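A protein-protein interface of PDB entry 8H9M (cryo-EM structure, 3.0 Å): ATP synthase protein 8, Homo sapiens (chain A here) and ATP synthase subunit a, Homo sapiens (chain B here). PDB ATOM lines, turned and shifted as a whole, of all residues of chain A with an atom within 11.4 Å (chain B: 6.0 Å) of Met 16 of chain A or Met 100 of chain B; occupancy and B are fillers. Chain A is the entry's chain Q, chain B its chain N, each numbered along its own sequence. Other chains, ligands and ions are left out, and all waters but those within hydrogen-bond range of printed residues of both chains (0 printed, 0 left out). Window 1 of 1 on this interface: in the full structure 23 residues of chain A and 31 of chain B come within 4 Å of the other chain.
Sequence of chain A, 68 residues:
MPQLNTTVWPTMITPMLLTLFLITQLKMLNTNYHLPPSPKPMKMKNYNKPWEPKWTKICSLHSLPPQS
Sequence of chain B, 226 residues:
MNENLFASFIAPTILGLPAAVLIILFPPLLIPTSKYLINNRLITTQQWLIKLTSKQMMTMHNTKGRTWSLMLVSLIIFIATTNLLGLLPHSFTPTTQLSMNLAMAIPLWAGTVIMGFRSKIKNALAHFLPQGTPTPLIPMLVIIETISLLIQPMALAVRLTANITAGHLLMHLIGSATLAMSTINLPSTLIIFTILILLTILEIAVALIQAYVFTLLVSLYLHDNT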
ATOM      1  N   PRO A   2       4.102  32.228   8.052  1.00  0.00           N
ATOM      2  CA  PRO A   2       4.413  33.044   9.233  1.00  0.00           C
ATOM      3  C   PRO A   2       5.804  32.797   9.781  1.00  0.00           C
ATOM      4  O   PRO A   2       6.313  33.637  10.533  1.00  0.00           O
ATOM      5  CB  PRO A   2       3.332  32.634  10.239  1.00  0.00           C
ATOM      6  CG  PRO A   2       2.947  31.261   9.828  1.00  0.00           C
ATOM      7  CD  PRO A   2       3.070  31.217   8.333  1.00  0.00           C
ATOM      8  N   GLN A   3       6.437  31.675   9.431  1.00  0.00           N
ATOM      9  CA  GLN A   3       7.810  31.429   9.852  1.00  0.00           C
ATOM     10  C   GLN A   3       8.779  32.449   9.274  1.00  0.00           C
ATOM     11  O   GLN A   3       9.890  32.595   9.793  1.00  0.00           O
ATOM     12  CB  GLN A   3       8.240  30.021   9.445  1.00  0.00           C
ATOM     13  CG  GLN A   3       7.760  28.934  10.381  1.00  0.00           C
ATOM     14  CD  GLN A   3       6.470  28.301   9.918  1.00  0.00           C
ATOM     15  OE1 GLN A   3       5.545  28.988   9.489  1.00  0.00           O
ATOM     16  NE2 GLN A   3       6.400  26.979  10.000  1.00  0.00           N
ATOM     17  N   LEU A   4       8.389  33.152   8.212  1.00  0.00           N
ATOM     18  CA  LEU A   4       9.229  34.171   7.605  1.00  0.00           C
ATOM     19  C   LEU A   4       8.902  35.578   8.084  1.00  0.00           C
ATOM     20  O   LEU A   4       9.557  36.531   7.651  1.00  0.00           O
ATOM     21  CB  LEU A   4       9.111  34.112   6.079  1.00  0.00           C
ATOM     22  CG  LEU A   4       9.360  32.730   5.476  1.00  0.00           C
ATOM     23  CD1 LEU A   4       8.881  32.671   4.035  1.00  0.00           C
ATOM     24  CD2 LEU A   4      10.832  32.366   5.573  1.00  0.00           C
ATOM     25  N   ASN A   5       7.914  35.732   8.960  1.00  0.00           N
ATOM     26  CA  ASN A   5       7.604  37.031   9.552  1.00  0.00           C
ATOM     27  C   ASN A   5       8.698  37.368  10.553  1.00  0.00           C
ATOM     28  O   ASN A   5       8.637  36.973  11.719  1.00  0.00           O
ATOM     29  CB  ASN A   5       6.234  37.001  10.217  1.00  0.00           C
ATOM     30  CG  ASN A   5       5.839  38.341  10.796  1.00  0.00           C
ATOM     31  OD1 ASN A   5       6.312  39.386  10.352  1.00  0.00           O
ATOM     32  ND2 ASN A   5       4.967  38.320  11.795  1.00  0.00           N
ATOM     33  N   THR A   6       9.704  38.111  10.102  1.00  0.00           N
ATOM     34  CA  THR A   6      10.890  38.394  10.898  1.00  0.00           C
ATOM     35  C   THR A   6      10.653  39.428  11.991  1.00  0.00           C
ATOM     36  O   THR A   6      11.622  39.893  12.598  1.00  0.00           O
ATOM     37  CB  THR A   6      12.030  38.861   9.989  1.00  0.00           C
ATOM     38  OG1 THR A   6      11.516  39.770   9.009  1.00  0.00           O
ATOM     39  CG2 THR A   6      12.666  37.677   9.284  1.00  0.00           C
ATOM     40  N   VAL A   8       8.495  38.975  14.797  1.00  0.00           N
ATOM     41  CA  VAL A   8       8.361  38.313  16.088  1.00  0.00           C
ATOM     42  C   VAL A   8       9.536  37.373  16.305  1.00  0.00           C
ATOM     43  O   VAL A   8       9.508  36.526  17.205  1.00  0.00           O
ATOM     44  CB  VAL A   8       7.028  37.553  16.191  1.00  0.00           C
ATOM     45  CG1 VAL A   8       5.860  38.499  15.986  1.00  0.00           C
ATOM     46  CG2 VAL A   8       6.987  36.424  15.177  1.00  0.00           C
ATOM     47  N   TRP A   9      10.574  37.510  15.483  1.00  0.00           N
ATOM     48  CA  TRP A   9      11.722  36.615  15.604  1.00  0.00           C
ATOM     49  C   TRP A   9      12.413  36.720  16.958  1.00  0.00           C
ATOM     50  O   TRP A   9      12.672  35.670  17.568  1.00  0.00           O
ATOM     51  CB  TRP A   9      12.692  36.855  14.443  1.00  0.00           C
ATOM     52  CG  TRP A   9      12.372  36.012  13.250  1.00  0.00           C
ATOM     53  CD1 TRP A   9      11.133  35.629  12.831  1.00  0.00           C
ATOM     54  CD2 TRP A   9      13.303  35.418  12.336  1.00  0.00           C
ATOM     55  NE1 TRP A   9      11.231  34.848  11.709  1.00  0.00           N
ATOM     56  CE2 TRP A   9      12.554  34.701  11.385  1.00  0.00           C
ATOM     57  CE3 TRP A   9      14.696  35.426  12.229  1.00  0.00           C
ATOM     58  CZ2 TRP A   9      13.147  34.002  10.340  1.00  0.00           C
ATOM     59  CZ3 TRP A   9      15.284  34.732  11.190  1.00  0.00           C
ATOM     60  CH2 TRP A   9      14.510  34.030  10.259  1.00  0.00           C
ATOM     61  N   PRO A  10      12.726  37.909  17.493  1.00  0.00           N
ATOM     62  CA  PRO A  10      13.328  37.950  18.839  1.00  0.00           C
ATOM     63  C   PRO A  10      12.490  37.258  19.898  1.00  0.00           C
ATOM     64  O   PRO A  10      13.044  36.575  20.770  1.00  0.00           O
ATOM     65  CB  PRO A  10      13.460  39.453  19.114  1.00  0.00           C
ATOM     66  CG  PRO A  10      13.582  40.059  17.772  1.00  0.00           C
ATOM     67  CD  PRO A  10      12.677  39.254  16.889  1.00  0.00           C
ATOM     68  N   THR A  11      11.163  37.402  19.833  1.00  0.00           N
ATOM     69  CA  THR A  11      10.285  36.767  20.813  1.00  0.00           C
ATOM     70  C   THR A  11      10.473  35.253  20.840  1.00  0.00           C
ATOM     71  O   THR A  11      10.191  34.610  21.856  1.00  0.00           O
ATOM     72  CB  THR A  11       8.829  37.132  20.509  1.00  0.00           C
ATOM     73  OG1 THR A  11       8.674  38.554  20.572  1.00  0.00           O
ATOM     74  CG2 THR A  11       7.876  36.495  21.509  1.00  0.00           C
ATOM     75  N   MET A  12      10.958  34.668  19.747  1.00  0.00           N
ATOM     76  CA  MET A  12      11.281  33.248  19.736  1.00  0.00           C
ATOM     77  C   MET A  12      12.720  32.969  20.138  1.00  0.00           C
ATOM     78  O   MET A  12      12.994  31.930  20.746  1.00  0.00           O
ATOM     79  CB  MET A  12      11.025  32.654  18.349  1.00  0.00           C
ATOM     80  CG  MET A  12       9.623  32.874  17.826  1.00  0.00           C
ATOM     81  SD  MET A  12       8.367  32.222  18.935  1.00  0.00           S
ATOM     82  CE  MET A  12       6.962  33.199  18.427  1.00  0.00           C
ATOM     83  N   ILE A  13      13.649  33.870  19.817  1.00  0.00           N
ATOM     84  CA  ILE A  13      15.054  33.600  20.097  1.00  0.00           C
ATOM     85  C   ILE A  13      15.356  33.773  21.579  1.00  0.00           C
ATOM     86  O   ILE A  13      16.099  32.981  22.167  1.00  0.00           O
ATOM     87  CB  ILE A  13      15.959  34.503  19.238  1.00  0.00           C
ATOM     88  CG1 ILE A  13      15.480  34.542  17.788  1.00  0.00           C
ATOM     89  CG2 ILE A  13      17.402  34.041  19.318  1.00  0.00           C
ATOM     90  CD1 ILE A  13      15.704  33.275  17.031  1.00  0.00           C
ATOM     91  N   THR A  14      14.787  34.804  22.206  1.00  0.00           N
ATOM     92  CA  THR A  14      15.224  35.166  23.554  1.00  0.00           C
ATOM     93  C   THR A  14      14.830  34.129  24.601  1.00  0.00           C
ATOM     94  O   THR A  14      15.723  33.651  25.322  1.00  0.00           O
ATOM     95  CB  THR A  14      14.712  36.564  23.908  1.00  0.00           C
ATOM     96  OG1 THR A  14      14.889  37.435  22.786  1.00  0.00           O
ATOM     97  CG2 THR A  14      15.475  37.122  25.093  1.00  0.00           C
ATOM     98  N   PRO A  15      13.559  33.737  24.752  1.00  0.00           N
ATOM     99  CA  PRO A  15      13.237  32.775  25.818  1.00  0.00           C
ATOM    100  C   PRO A  15      13.859  31.408  25.612  1.00  0.00           C
ATOM    101  O   PRO A  15      14.197  30.744  26.600  1.00  0.00           O
ATOM    102  CB  PRO A  15      11.705  32.711  25.784  1.00  0.00           C
ATOM    103  CG  PRO A  15      11.349  33.098  24.421  1.00  0.00           C
ATOM    104  CD  PRO A  15      12.348  34.133  24.015  1.00  0.00           C
ATOM    105  N   MET A  16      14.026  30.965  24.363  1.00  0.00           N
ATOM    106  CA  MET A  16      14.671  29.678  24.118  1.00  0.00           C
ATOM    107  C   MET A  16      16.045  29.625  24.766  1.00  0.00           C
ATOM    108  O   MET A  16      16.380  28.660  25.463  1.00  0.00           O
ATOM    109  CB  MET A  16      14.786  29.416  22.618  1.00  0.00           C
ATOM    110  CG  MET A  16      15.379  28.058  22.287  1.00  0.00           C
ATOM    111  SD  MET A  16      17.178  28.041  22.212  1.00  0.00           S
ATOM    112  CE  MET A  16      17.461  29.143  20.839  1.00  0.00           C
ATOM    113  N   LEU A  17      16.865  30.651  24.531  1.00  0.00           N
ATOM    114  CA  LEU A  17      18.161  30.722  25.192  1.00  0.00           C
ATOM    115  C   LEU A  17      18.006  30.738  26.704  1.00  0.00           C
ATOM    116  O   LEU A  17      18.806  30.124  27.418  1.00  0.00           O
ATOM    117  CB  LEU A  17      18.921  31.958  24.717  1.00  0.00           C
ATOM    118  CG  LEU A  17      19.121  32.056  23.206  1.00  0.00           C
ATOM    119  CD1 LEU A  17      19.591  33.445  22.817  1.00  0.00           C
ATOM    120  CD2 LEU A  17      20.104  31.003  22.731  1.00  0.00           C
ATOM    121  N   LEU A  18      16.977  31.417  27.207  1.00  0.00           N
ATOM    122  CA  LEU A  18      16.697  31.415  28.634  1.00  0.00           C
ATOM    123  C   LEU A  18      16.230  30.053  29.126  1.00  0.00           C
ATOM    124  O   LEU A  18      16.349  29.763  30.320  1.00  0.00           O
ATOM    125  CB  LEU A  18      15.649  32.483  28.952  1.00  0.00           C
ATOM    126  CG  LEU A  18      15.149  32.625  30.387  1.00  0.00           C
ATOM    127  CD1 LEU A  18      16.299  32.973  31.314  1.00  0.00           C
ATOM    128  CD2 LEU A  18      14.058  33.677  30.458  1.00  0.00           C
ATOM    129  N   THR A  19      15.725  29.208  28.232  1.00  0.00           N
ATOM    130  CA  THR A  19      15.223  27.886  28.576  1.00  0.00           C
ATOM    131  C   THR A  19      16.202  26.773  28.236  1.00  0.00           C
ATOM    132  O   THR A  19      16.381  25.844  29.029  1.00  0.00           O
ATOM    133  CB  THR A  19      13.893  27.632  27.859  1.00  0.00           C
ATOM    134  OG1 THR A  19      12.872  28.448  28.439  1.00  0.00           O
ATOM    135  CG2 THR A  19      13.488  26.185  27.974  1.00  0.00           C
ATOM    136  N   LEU A  20      16.854  26.852  27.078  1.00  0.00           N
ATOM    137  CA  LEU A  20      17.775  25.800  26.673  1.00  0.00           C
ATOM    138  C   LEU A  20      19.116  25.900  27.385  1.00  0.00           C
ATOM    139  O   LEU A  20      19.738  24.871  27.670  1.00  0.00           O
ATOM    140  CB  LEU A  20      17.985  25.844  25.160  1.00  0.00           C
ATOM    141  CG  LEU A  20      19.058  24.920  24.595  1.00  0.00           C
ATOM    142  CD1 LEU A  20      18.675  23.481  24.838  1.00  0.00           C
ATOM    143  CD2 LEU A  20      19.266  25.179  23.118  1.00  0.00           C
ATOM    144  N   PHE A  21      19.576  27.113  27.692  1.00  0.00           N
ATOM    145  CA  PHE A  21      20.926  27.308  28.196  1.00  0.00           C
ATOM    146  C   PHE A  21      21.002  27.614  29.685  1.00  0.00           C
ATOM    147  O   PHE A  21      22.093  27.519  30.255  1.00  0.00           O
ATOM    148  CB  PHE A  21      21.623  28.431  27.415  1.00  0.00           C
ATOM    149  CG  PHE A  21      22.150  27.998  26.080  1.00  0.00           C
ATOM    150  CD1 PHE A  21      23.410  27.448  25.964  1.00  0.00           C
ATOM    151  CD2 PHE A  21      21.378  28.129  24.941  1.00  0.00           C
ATOM    152  CE1 PHE A  21      23.894  27.046  24.738  1.00  0.00           C
ATOM    153  CE2 PHE A  21      21.855  27.723  23.711  1.00  0.00           C
ATOM    154  CZ  PHE A  21      23.115  27.181  23.610  1.00  0.00           C
ATOM    155  N   LEU A  22      19.899  27.987  30.332  1.00  0.00           N
ATOM    156  CA  LEU A  22      19.934  28.256  31.766  1.00  0.00           C
ATOM    157  C   LEU A  22      19.015  27.337  32.557  1.00  0.00           C
ATOM    158  O   LEU A  22      19.481  26.656  33.475  1.00  0.00           O
ATOM    159  CB  LEU A  22      19.589  29.729  32.028  1.00  0.00           C
ATOM    160  CG  LEU A  22      19.786  30.283  33.443  1.00  0.00           C
ATOM    161  CD1 LEU A  22      20.126  31.756  33.370  1.00  0.00           C
ATOM    162  CD2 LEU A  22      18.551  30.085  34.307  1.00  0.00           C
ATOM    163  N   ILE A  23      17.725  27.280  32.228  1.00  0.00           N
ATOM    164  CA  ILE A  23      16.768  26.624  33.114  1.00  0.00           C
ATOM    165  C   ILE A  23      16.899  25.109  33.026  1.00  0.00           C
ATOM    166  O   ILE A  23      17.023  24.420  34.046  1.00  0.00           O
ATOM    167  CB  ILE A  23      15.337  27.084  32.791  1.00  0.00           C
ATOM    168  CG1 ILE A  23      15.188  28.578  33.070  1.00  0.00           C
ATOM    169  CG2 ILE A  23      14.332  26.295  33.604  1.00  0.00           C
ATOM    170  CD1 ILE A  23      13.814  29.117  32.765  1.00  0.00           C
ATOM    171  N   THR A  24      16.868  24.566  31.809  1.00  0.00           N
ATOM    172  CA  THR A  24      16.940  23.118  31.659  1.00  0.00           C
ATOM    173  C   THR A  24      18.281  22.585  32.143  1.00  0.00           C
ATOM    174  O   THR A  24      18.352  21.504  32.740  1.00  0.00           O
ATOM    175  CB  THR A  24      16.695  22.729  30.205  1.00  0.00           C
ATOM    176  OG1 THR A  24      15.524  23.396  29.726  1.00  0.00           O
ATOM    177  CG2 THR A  24      16.478  21.234  30.095  1.00  0.00           C
ATOM    178  N   GLN A  25      19.355  23.340  31.921  1.00  0.00           N
ATOM    179  CA  GLN A  25      20.657  22.908  32.413  1.00  0.00           C
ATOM    180  C   GLN A  25      20.729  22.992  33.934  1.00  0.00           C
ATOM    181  O   GLN A  25      21.353  22.142  34.579  1.00  0.00           O
ATOM    182  CB  GLN A  25      21.762  23.732  31.755  1.00  0.00           C
ATOM    183  CG  GLN A  25      21.869  23.474  30.265  1.00  0.00           C
ATOM    184  CD  GLN A  25      22.959  24.272  29.593  1.00  0.00           C
ATOM    185  OE1 GLN A  25      23.624  25.087  30.221  1.00  0.00           O
ATOM    186  NE2 GLN A  25      23.150  24.037  28.302  1.00  0.00           N
ATOM    187  N   LEU A  26      20.087  24.002  34.527  1.00  0.00           N
ATOM    188  CA  LEU A  26      20.027  24.081  35.981  1.00  0.00           C
ATOM    189  C   LEU A  26      19.190  22.964  36.583  1.00  0.00           C
ATOM    190  O   LEU A  26      19.409  22.596  37.741  1.00  0.00           O
ATOM    191  CB  LEU A  26      19.472  25.434  36.423  1.00  0.00           C
ATOM    192  CG  LEU A  26      20.491  26.566  36.548  1.00  0.00           C
ATOM    193  CD1 LEU A  26      19.864  27.766  37.229  1.00  0.00           C
ATOM    194  CD2 LEU A  26      21.714  26.096  37.307  1.00  0.00           C
ATOM    195  N   ILE B  24       7.292  28.735  25.575  1.00  0.00           N
ATOM    196  CA  ILE B  24       8.650  28.213  25.490  1.00  0.00           C
ATOM    197  C   ILE B  24       9.220  27.947  26.879  1.00  0.00           C
ATOM    198  O   ILE B  24      10.045  27.042  27.051  1.00  0.00           O
ATOM    199  CB  ILE B  24       9.541  29.172  24.682  1.00  0.00           C
ATOM    200  CG1 ILE B  24       9.017  29.307  23.254  1.00  0.00           C
ATOM    201  CG2 ILE B  24      10.973  28.677  24.638  1.00  0.00           C
ATOM    202  CD1 ILE B  24       9.735  30.350  22.441  1.00  0.00           C
ATOM    203  N   PHE B  78      14.918  19.251  26.064  1.00  0.00           N
ATOM    204  CA  PHE B  78      14.124  20.412  25.680  1.00  0.00           C
ATOM    205  C   PHE B  78      13.390  20.171  24.369  1.00  0.00           C
ATOM    206  O   PHE B  78      12.180  20.411  24.272  1.00  0.00           O
ATOM    207  CB  PHE B  78      15.020  21.644  25.578  1.00  0.00           C
ATOM    208  CG  PHE B  78      14.358  22.820  24.933  1.00  0.00           C
ATOM    209  CD1 PHE B  78      13.355  23.507  25.584  1.00  0.00           C
ATOM    210  CD2 PHE B  78      14.745  23.245  23.679  1.00  0.00           C
ATOM    211  CE1 PHE B  78      12.747  24.590  24.993  1.00  0.00           C
ATOM    212  CE2 PHE B  78      14.141  24.327  23.086  1.00  0.00           C
ATOM    213  CZ  PHE B  78      13.141  25.000  23.745  1.00  0.00           C
ATOM    214  N   THR B  82       9.312  19.842  24.007  1.00  0.00           N
ATOM    215  CA  THR B  82       8.621  20.820  23.173  1.00  0.00           C
ATOM    216  C   THR B  82       7.834  20.134  22.064  1.00  0.00           C
ATOM    217  O   THR B  82       6.650  20.427  21.853  1.00  0.00           O
ATOM    218  CB  THR B  82       9.620  21.814  22.586  1.00  0.00           C
ATOM    219  OG1 THR B  82      10.067  22.706  23.612  1.00  0.00           O
ATOM    220  CG2 THR B  82       8.971  22.620  21.491  1.00  0.00           C
ATOM    221  N   PRO B  94       6.780  25.699  19.342  1.00  0.00           N
ATOM    222  CA  PRO B  94       7.854  26.625  18.960  1.00  0.00           C
ATOM    223  C   PRO B  94       8.951  25.988  18.127  1.00  0.00           C
ATOM    224  O   PRO B  94       9.815  26.717  17.627  1.00  0.00           O
ATOM    225  CB  PRO B  94       8.389  27.120  20.308  1.00  0.00           C
ATOM    226  CG  PRO B  94       8.021  26.061  21.268  1.00  0.00           C
ATOM    227  CD  PRO B  94       6.722  25.493  20.798  1.00  0.00           C
ATOM    228  N   THR B  95       8.959  24.666  17.959  1.00  0.00           N
ATOM    229  CA  THR B  95       9.887  24.060  17.013  1.00  0.00           C
ATOM    230  C   THR B  95       9.373  24.096  15.583  1.00  0.00           C
ATOM    231  O   THR B  95      10.120  23.745  14.666  1.00  0.00           O
ATOM    232  CB  THR B  95      10.201  22.615  17.403  1.00  0.00           C
ATOM    233  OG1 THR B  95       8.988  21.925  17.716  1.00  0.00           O
ATOM    234  CG2 THR B  95      11.132  22.579  18.596  1.00  0.00           C
ATOM    235  N   GLN B  97       8.787  26.929  14.354  1.00  0.00           N
ATOM    236  CA  GLN B  97       9.330  28.216  13.954  1.00  0.00           C
ATOM    237  C   GLN B  97      10.765  28.040  13.482  1.00  0.00           C
ATOM    238  O   GLN B  97      11.559  27.355  14.133  1.00  0.00           O
ATOM    239  CB  GLN B  97       9.277  29.205  15.117  1.00  0.00           C
ATOM    240  CG  GLN B  97       7.888  29.439  15.666  1.00  0.00           C
ATOM    241  CD  GLN B  97       6.984  30.126  14.670  1.00  0.00           C
ATOM    242  OE1 GLN B  97       7.369  31.110  14.043  1.00  0.00           O
ATOM    243  NE2 GLN B  97       5.771  29.613  14.520  1.00  0.00           N
ATOM    244  N   LEU B  98      11.093  28.657  12.346  1.00  0.00           N
ATOM    245  CA  LEU B  98      12.471  28.645  11.876  1.00  0.00           C
ATOM    246  C   LEU B  98      13.382  29.458  12.780  1.00  0.00           C
ATOM    247  O   LEU B  98      14.588  29.196  12.827  1.00  0.00           O
ATOM    248  CB  LEU B  98      12.539  29.172  10.443  1.00  0.00           C
ATOM    249  CG  LEU B  98      13.914  29.168   9.775  1.00  0.00           C
ATOM    250  CD1 LEU B  98      14.400  27.748   9.566  1.00  0.00           C
ATOM    251  CD2 LEU B  98      13.875  29.924   8.460  1.00  0.00           C
ATOM    252  N   SER B  99      12.826  30.424  13.512  1.00  0.00           N
ATOM    253  CA  SER B  99      13.624  31.248  14.413  1.00  0.00           C
ATOM    254  C   SER B  99      14.289  30.402  15.488  1.00  0.00           C
ATOM    255  O   SER B  99      15.515  30.410  15.638  1.00  0.00           O
ATOM    256  CB  SER B  99      12.735  32.305  15.057  1.00  0.00           C
ATOM    257  OG  SER B  99      12.406  33.306  14.127  1.00  0.00           O
ATOM    258  N   MET B 100      13.478  29.687  16.268  1.00  0.00           N
ATOM    259  CA  MET B 100      14.006  28.905  17.377  1.00  0.00           C
ATOM    260  C   MET B 100      14.964  27.829  16.888  1.00  0.00           C
ATOM    261  O   MET B 100      16.013  27.596  17.499  1.00  0.00           O
ATOM    262  CB  MET B 100      12.854  28.281  18.160  1.00  0.00           C
ATOM    263  CG  MET B 100      13.099  28.204  19.640  1.00  0.00           C
ATOM    264  SD  MET B 100      11.871  27.210  20.491  1.00  0.00           S
ATOM    265  CE  MET B 100      12.532  25.574  20.208  1.00  0.00           C
ATOM    266  N   ASN B 101      14.632  27.172  15.779  1.00  0.00           N
ATOM    267  CA  ASN B 101      15.492  26.106  15.281  1.00  0.00           C
ATOM    268  C   ASN B 101      16.813  26.656  14.765  1.00  0.00           C
ATOM    269  O   ASN B 101      17.869  26.052  14.983  1.00  0.00           O
ATOM    270  CB  ASN B 101      14.764  25.322  14.196  1.00  0.00           C
ATOM    271  CG  ASN B 101      13.379  24.907  14.624  1.00  0.00           C
ATOM    272  OD1 ASN B 101      13.196  24.346  15.701  1.00  0.00           O
ATOM    273  ND2 ASN B 101      12.391  25.193  13.790  1.00  0.00           N
ATOM    274  N   LEU B 102      16.782  27.806  14.089  1.00  0.00           N
ATOM    275  CA  LEU B 102      18.025  28.423  13.641  1.00  0.00           C
ATOM    276  C   LEU B 102      18.876  28.857  14.825  1.00  0.00           C
ATOM    277  O   LEU B 102      20.097  28.671  14.822  1.00  0.00           O
ATOM    278  CB  LEU B 102      17.724  29.613  12.733  1.00  0.00           C
ATOM    279  CG  LEU B 102      17.682  29.332  11.231  1.00  0.00           C
ATOM    280  CD1 LEU B 102      17.510  30.627  10.457  1.00  0.00           C
ATOM    281  CD2 LEU B 102      18.939  28.606  10.787  1.00  0.00           C
ATOM    282  N   ALA B 103      18.249  29.430  15.852  1.00  0.00           N
ATOM    283  CA  ALA B 103      18.992  29.871  17.023  1.00  0.00           C
ATOM    284  C   ALA B 103      19.426  28.718  17.915  1.00  0.00           C
ATOM    285  O   ALA B 103      20.218  28.934  18.837  1.00  0.00           O
ATOM    286  CB  ALA B 103      18.159  30.859  17.830  1.00  0.00           C
ATOM    287  N   MET B 104      18.900  27.518  17.693  1.00  0.00           N
ATOM    288  CA  MET B 104      19.429  26.327  18.344  1.00  0.00           C
ATOM    289  C   MET B 104      20.535  25.668  17.538  1.00  0.00           C
ATOM    290  O   MET B 104      21.449  25.077  18.124  1.00  0.00           O
ATOM    291  CB  MET B 104      18.313  25.308  18.581  1.00  0.00           C
ATOM    292  CG  MET B 104      17.546  25.498  19.869  1.00  0.00           C
ATOM    293  SD  MET B 104      16.526  24.073  20.269  1.00  0.00           S
ATOM    294  CE  MET B 104      15.697  23.816  18.707  1.00  0.00           C
ATOM    295  N   ALA B 105      20.477  25.760  16.211  1.00  0.00           N
ATOM    296  CA  ALA B 105      21.410  25.047  15.348  1.00  0.00           C
ATOM    297  C   ALA B 105      22.680  25.840  15.069  1.00  0.00           C
ATOM    298  O   ALA B 105      23.778  25.276  15.098  1.00  0.00           O
ATOM    299  CB  ALA B 105      20.724  24.681  14.030  1.00  0.00           C
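The side-chain hydroxyl (OG1) of Thr 19 of chain A is in hydrogen-bond range of the backbone carbonyl oxygen (O) of Ile 24 of chain B (3.4 Å). The side-chain hydroxyl (OG) of Ser 99 of chain B sits close to the indole nitrogen (NE1) of Trp 9 of chain A, at 3.1 Å.
The backbone carbonyl oxygen of Phe 78 of chain B sits at hydrogen-bond distance from the side-chain hydroxyl of Thr 82 of chain B. The backbone carbonyl oxygen (O) of Gln 3 of chain A lies within hydrogen-bond range of the indole nitrogen (NE1) of Trp 9 of chain A. O of Asn 5 of chain A lies close to NE1 of Trp 9 of chain A, at 3.4 Å. The backbone carbonyl oxygen of Pro 15 of chain A lies within hydrogen-bond range of the side-chain hydroxyl of Thr 19 of chain A (3.2 Å). O of Thr 19 of chain A lies within hydrogen-bond range of OG1 of Thr 24 of chain A, at 2.7 Å.
Among the printed residues, pairs that only touch across the chains: Ile 13 of chain A with Ser 99 of chain B, Met 16 of chain A with Ala 103 of chain B, Thr 19 of chain A with Phe 78 of chain B, Met 16 of chain A with Met 104 of chain B, Met 16 of chain A with Met 100 of chain B, Ile 13 of chain A with Ala 103 of chain B, Leu 20 of chain A with Met 104 of chain B, Met 12 of chain A with Ser 99 of chain B, Pro 15 of chain A with Ile 24 of chain B, Met 16 of chain A with Ile 24 of chain B, Gln 3 of chain A with Leu 98 of chain B, Met 12 of chain A with Met 100 of chain B, Gln 3 of chain A with Gln 97 of chain B and Met 12 of chain A with Ile 24 of chain B.
Thr 6 of chain A touches none of the printed residues of chain B. Printed residues of chain B within 4 Å of Pro 15 of chain A: Ile 24. Of the printed residues of chain B, Met 16 of chain A touches Ile 24 (3.8 Å), Met 100 (3.5 Å), Ala 103 (3.4 Å) and Met 104 (3.5 Å). Of the printed residues of chain A, Ile 24 of chain B touches Met 12 (3.999 Å), Pro 15 (3.8 Å), Met 16 (3.8 Å) and Thr 19 (3.4 Å). No residue of chain A comes within 4 Å of Thr 95 of chain B. Of the printed residues of chain A, Gln 97 of chain B touches Gln 3 (3.97 Å). Of chain A, only Trp 9 (2.8 Å), Met 12 (3.7 Å) and Ile 13 (3.2 Å) come within 4 Å of Ser 99 of chain B. Of chain A, only Met 12 (3.9 Å) and Met 16 (3.5 Å) come within 4 Å of Met 100 of chain B. No residue of chain A comes within 4 Å of Asn 101 of chain B. No residue of chain A comes within 4 Å of Leu 102 of chain B. Of the printed residues of chain A, Ala 103 of chain B touches Ile 13 (3.5 Å) and Met 16 (3.4 Å). The nearest printed residue of chain B that does not touch Met 16 of chain A is Phe 78 of chain B (4.01 Å). The nearest residue of chain A that does not touch Met 100 of chain B is Ile 13 of chain A (4.3 Å).
Of the 24 printed residues of chain A, 8 touch a printed residue of chain B. Hydrophobic or aromatic side chains of chain A within 4 Å of the printed part of chain B: Trp 9, Met 12, Ile 13, Pro 15, Met 16 and Leu 20. Hydrophobic or aromatic side chains of chain B within 4 Å of the printed part of chain A: Ile 24, Phe 78, Met 100, Ala 103 and Met 104.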
